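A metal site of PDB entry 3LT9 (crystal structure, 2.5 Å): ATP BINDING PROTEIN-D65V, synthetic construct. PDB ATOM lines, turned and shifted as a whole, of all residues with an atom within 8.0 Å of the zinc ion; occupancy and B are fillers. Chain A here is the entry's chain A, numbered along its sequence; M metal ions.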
ATOM      1  N   PRO A  24      12.767   1.326  -5.137  1.00  0.00           N
ATOM      2  CA  PRO A  24      12.505   0.502  -3.949  1.00  0.00           C
ATOM      3  C   PRO A  24      11.486   1.184  -3.026  1.00  0.00           C
ATOM      4  O   PRO A  24      11.071   2.316  -3.309  1.00  0.00           O
ATOM      5  CB  PRO A  24      13.862   0.454  -3.245  1.00  0.00           C
ATOM      6  CG  PRO A  24      14.573   1.696  -3.712  1.00  0.00           C
ATOM      7  CD  PRO A  24      14.101   1.960  -5.103  1.00  0.00           C
ATOM      8  N   CYS A  25      11.088   0.490  -1.959  1.00  0.00           N
ATOM      9  CA  CYS A  25      10.231   1.012  -0.905  1.00  0.00           C
ATOM     10  C   CYS A  25      10.417   2.521  -0.631  1.00  0.00           C
ATOM     11  O   CYS A  25      11.551   2.947  -0.416  1.00  0.00           O
ATOM     12  CB  CYS A  25      10.567   0.247   0.371  1.00  0.00           C
ATOM     13  SG  CYS A  25       9.574   0.731   1.773  1.00  0.00           S
ATOM     14  N   VAL A  26       9.351   3.322  -0.617  1.00  0.00           N
ATOM     15  CA  VAL A  26       9.545   4.752  -0.346  1.00  0.00           C
ATOM     16  C   VAL A  26      10.043   4.998   1.089  1.00  0.00           C
ATOM     17  O   VAL A  26      10.574   6.063   1.391  1.00  0.00           O
ATOM     18  CB  VAL A  26       8.252   5.613  -0.542  1.00  0.00           C
ATOM     19  CG1 VAL A  26       7.848   5.728  -2.007  1.00  0.00           C
ATOM     20  CG2 VAL A  26       7.121   5.083   0.305  1.00  0.00           C
ATOM     21  N   LYS A  27       9.850   4.034   1.983  1.00  0.00           N
ATOM     22  CA  LYS A  27      10.100   4.295   3.386  1.00  0.00           C
ATOM     23  C   LYS A  27      11.484   3.875   3.824  1.00  0.00           C
ATOM     24  O   LYS A  27      12.222   4.690   4.385  1.00  0.00           O
ATOM     25  CB  LYS A  27       9.027   3.679   4.283  1.00  0.00           C
ATOM     26  CG  LYS A  27       9.277   3.872   5.760  1.00  0.00           C
ATOM     27  CD  LYS A  27       9.386   5.340   6.116  1.00  0.00           C
ATOM     28  CE  LYS A  27       9.768   5.502   7.575  1.00  0.00           C
ATOM     29  NZ  LYS A  27       9.737   6.941   7.965  1.00  0.00           N
ATOM     30  N   CYS A  28      11.844   2.621   3.590  1.00  0.00           N
ATOM     31  CA  CYS A  28      13.200   2.168   3.936  1.00  0.00           C
ATOM     32  C   CYS A  28      14.176   2.371   2.794  1.00  0.00           C
ATOM     33  O   CYS A  28      15.367   2.316   3.005  1.00  0.00           O
ATOM     34  CB  CYS A  28      13.211   0.700   4.354  1.00  0.00           C
ATOM     35  SG  CYS A  28      12.873  -0.437   2.954  1.00  0.00           S
ATOM     36  N   LYS A  29      13.675   2.580   1.574  1.00  0.00           N
ATOM     37  CA  LYS A  29      14.573   2.890   0.458  1.00  0.00           C
ATOM     38  C   LYS A  29      15.438   1.753  -0.080  1.00  0.00           C
ATOM     39  O   LYS A  29      16.068   1.951  -1.096  1.00  0.00           O
ATOM     40  CB  LYS A  29      15.544   3.986   0.860  1.00  0.00           C
ATOM     41  CG  LYS A  29      14.942   5.075   1.666  1.00  0.00           C
ATOM     42  CD  LYS A  29      14.306   6.064   0.793  1.00  0.00           C
ATOM     43  CE  LYS A  29      13.809   7.228   1.624  1.00  0.00           C
ATOM     44  NZ  LYS A  29      13.121   8.151   0.672  1.00  0.00           N
ATOM     45  N   VAL A  30      15.515   0.605   0.599  1.00  0.00           N
ATOM     46  CA  VAL A  30      16.272  -0.556   0.069  1.00  0.00           C
ATOM     47  C   VAL A  30      15.383  -1.719  -0.417  1.00  0.00           C
ATOM     48  O   VAL A  30      15.487  -2.155  -1.569  1.00  0.00           O
ATOM     49  CB  VAL A  30      17.272  -1.108   1.090  1.00  0.00           C
ATOM     50  CG1 VAL A  30      18.286  -1.997   0.374  1.00  0.00           C
ATOM     51  CG2 VAL A  30      18.001   0.032   1.778  1.00  0.00           C
ATOM     52  N   ALA A  31      14.523  -2.268   0.442  1.00  0.00           N
ATOM     53  CA  ALA A  31      13.647  -3.317  -0.012  1.00  0.00           C
ATOM     54  C   ALA A  31      12.793  -2.911  -1.222  1.00  0.00           C
ATOM     55  O   ALA A  31      12.427  -1.742  -1.425  1.00  0.00           O
ATOM     56  CB  ALA A  31      12.767  -3.798   1.099  1.00  0.00           C
ATOM     57  N   PRO A  32      12.488  -3.885  -2.066  1.00  0.00           N
ATOM     58  CA  PRO A  32      11.565  -3.617  -3.148  1.00  0.00           C
ATOM     59  C   PRO A  32      10.146  -3.562  -2.615  1.00  0.00           C
ATOM     60  O   PRO A  32       9.874  -4.008  -1.493  1.00  0.00           O
ATOM     61  CB  PRO A  32      11.767  -4.809  -4.083  1.00  0.00           C
ATOM     62  CG  PRO A  32      12.342  -5.892  -3.203  1.00  0.00           C
ATOM     63  CD  PRO A  32      13.151  -5.194  -2.178  1.00  0.00           C
ATOM     64  N   ARG A  33       9.248  -2.981  -3.396  1.00  0.00           N
ATOM     65  CA  ARG A  33       7.879  -2.729  -2.911  1.00  0.00           C
ATOM     66  C   ARG A  33       7.002  -3.989  -2.866  1.00  0.00           C
ATOM     67  O   ARG A  33       7.205  -4.961  -3.634  1.00  0.00           O
ATOM     68  CB  ARG A  33       7.206  -1.667  -3.782  1.00  0.00           C
ATOM     69  CG  ARG A  33       7.733  -0.295  -3.543  1.00  0.00           C
ATOM     70  CD  ARG A  33       7.359   0.607  -4.693  1.00  0.00           C
ATOM     71  NE  ARG A  33       8.221   1.780  -4.678  1.00  0.00           N
ATOM     72  CZ  ARG A  33       7.828   2.983  -5.075  1.00  0.00           C
ATOM     73  NH1 ARG A  33       6.581   3.157  -5.522  1.00  0.00           N
ATOM     74  NH2 ARG A  33       8.672   4.002  -5.019  1.00  0.00           N
ATOM     75  N   ASN A  34       6.023  -3.982  -1.968  1.00  0.00           N
ATOM     76  CA  ASN A  34       4.982  -4.976  -2.081  1.00  0.00           C
ATOM     77  C   ASN A  34       4.176  -4.759  -3.372  1.00  0.00           C
ATOM     78  O   ASN A  34       4.208  -3.668  -3.942  1.00  0.00           O
ATOM     79  CB  ASN A  34       4.058  -4.967  -0.881  1.00  0.00           C
ATOM     80  CG  ASN A  34       3.331  -6.288  -0.711  1.00  0.00           C
ATOM     81  OD1 ASN A  34       3.659  -7.298  -1.354  1.00  0.00           O
ATOM     82  ND2 ASN A  34       2.348  -6.298   0.159  1.00  0.00           N
ATOM     83  N   ASN A  46       3.368   1.440  -2.367  1.00  0.00           N
ATOM     84  CA  ASN A  46       4.501   2.322  -2.151  1.00  0.00           C
ATOM     85  C   ASN A  46       5.606   1.744  -1.236  1.00  0.00           C
ATOM     86  O   ASN A  46       6.769   2.159  -1.316  1.00  0.00           O
ATOM     87  CB  ASN A  46       4.025   3.698  -1.633  1.00  0.00           C
ATOM     88  CG  ASN A  46       2.979   4.326  -2.525  1.00  0.00           C
ATOM     89  OD1 ASN A  46       2.939   4.093  -3.759  1.00  0.00           O
ATOM     90  ND2 ASN A  46       2.121   5.149  -1.930  1.00  0.00           N
ATOM     91  N   MET A  47       5.247   0.793  -0.361  1.00  0.00           N
ATOM     92  CA  MET A  47       6.217   0.254   0.608  1.00  0.00           C
ATOM     93  C   MET A  47       6.380  -1.266   0.557  1.00  0.00           C
ATOM     94  O   MET A  47       5.491  -1.972   0.059  1.00  0.00           O
ATOM     95  CB  MET A  47       5.803   0.635   2.011  1.00  0.00           C
ATOM     96  CG  MET A  47       5.964   2.099   2.356  1.00  0.00           C
ATOM     97  SD  MET A  47       5.556   2.407   4.110  1.00  0.00           S
ATOM     98  CE  MET A  47       3.749   2.183   4.089  1.00  0.00           C
ATOM     99  N   CYS A  48       7.491  -1.771   1.079  1.00  0.00           N
ATOM    100  CA  CYS A  48       7.622  -3.237   1.201  1.00  0.00           C
ATOM    101  C   CYS A  48       6.654  -3.643   2.295  1.00  0.00           C
ATOM    102  O   CYS A  48       6.028  -2.761   2.910  1.00  0.00           O
ATOM    103  CB  CYS A  48       9.048  -3.637   1.556  1.00  0.00           C
ATOM    104  SG  CYS A  48       9.593  -3.009   3.162  1.00  0.00           S
ATOM    105  N   LYS A  49       6.503  -4.940   2.539  1.00  0.00           N
ATOM    106  CA  LYS A  49       5.506  -5.367   3.526  1.00  0.00           C
ATOM    107  C   LYS A  49       5.952  -5.025   4.946  1.00  0.00           C
ATOM    108  O   LYS A  49       5.109  -4.649   5.788  1.00  0.00           O
ATOM    109  CB  LYS A  49       5.224  -6.859   3.415  1.00  0.00           C
ATOM    110  CG  LYS A  49       4.270  -7.447   4.454  1.00  0.00           C
ATOM    111  CD  LYS A  49       2.912  -7.685   3.833  1.00  0.00           C
ATOM    112  CE  LYS A  49       1.922  -8.284   4.827  1.00  0.00           C
ATOM    113  NZ  LYS A  49       2.471  -9.548   5.444  1.00  0.00           N
ATOM    114  N   THR A  50       7.259  -5.153   5.210  1.00  0.00           N
ATOM    115  CA  THR A  50       7.781  -4.894   6.532  1.00  0.00           C
ATOM    116  C   THR A  50       7.502  -3.458   6.970  1.00  0.00           C
ATOM    117  O   THR A  50       7.045  -3.226   8.099  1.00  0.00           O
ATOM    118  CB  THR A  50       9.295  -5.160   6.618  1.00  0.00           C
ATOM    119  OG1 THR A  50       9.602  -6.489   6.178  1.00  0.00           O
ATOM    120  CG2 THR A  50       9.766  -4.984   8.076  1.00  0.00           C
ATOM    121  N   CYS A  51       7.746  -2.497   6.079  1.00  0.00           N
ATOM    122  CA  CYS A  51       7.541  -1.087   6.402  1.00  0.00           C
ATOM    123  C   CYS A  51       6.071  -0.719   6.400  1.00  0.00           C
ATOM    124  O   CYS A  51       5.655   0.153   7.150  1.00  0.00           O
ATOM    125  CB  CYS A  51       8.329  -0.153   5.451  1.00  0.00           C
ATOM    126  SG  CYS A  51      10.157  -0.274   5.580  1.00  0.00           S
ATOM    127  N   PHE A  52       5.262  -1.376   5.572  1.00  0.00           N
ATOM    128  CA  PHE A  52       3.827  -1.097   5.661  1.00  0.00           C
ATOM    129  C   PHE A  52       3.246  -1.510   7.030  1.00  0.00           C
ATOM    130  O   PHE A  52       2.564  -0.710   7.687  1.00  0.00           O
ATOM    131  CB  PHE A  52       3.067  -1.760   4.539  1.00  0.00           C
ATOM    132  CG  PHE A  52       1.577  -1.551   4.627  1.00  0.00           C
ATOM    133  CD1 PHE A  52       1.026  -0.299   4.444  1.00  0.00           C
ATOM    134  CD2 PHE A  52       0.718  -2.634   4.907  1.00  0.00           C
ATOM    135  CE1 PHE A  52      -0.360  -0.096   4.526  1.00  0.00           C
ATOM    136  CE2 PHE A  52      -0.656  -2.443   4.990  1.00  0.00           C
ATOM    137  CZ  PHE A  52      -1.201  -1.168   4.799  1.00  0.00           C
HETATM  138 ZN    ZN M   1      10.644  -0.705   3.290  1.00  0.00          ZN
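The backbone NH (N) of Ala 31 sits close to the side-chain sulfur (SG) of Cys 28, 3.5 Å away.
SG of Cys 28 sits close to N of Val 30 (3.7 Å).
The backbone NH of Cys 25 is in hydrogen-bond range of the backbone carbonyl oxygen of Ala 31 (2.7 Å).
The side-chain sulfur of Cys 25 sits close to the backbone NH of Lys 27 (3.3 Å).
SG of Cys 48 sits close to N of Thr 50 (3.8 Å).
Four residues have an atom within 4 Å of the zinc ion: Cys 25, Cys 28, Cys 48 and Cys 51.
The zinc ion is bound by SG of Cys 28 (2.3 Å), SG of Cys 25 (2.3 Å), SG of Cys 51 (2.4 Å) and SG of Cys 48 (2.5 Å).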
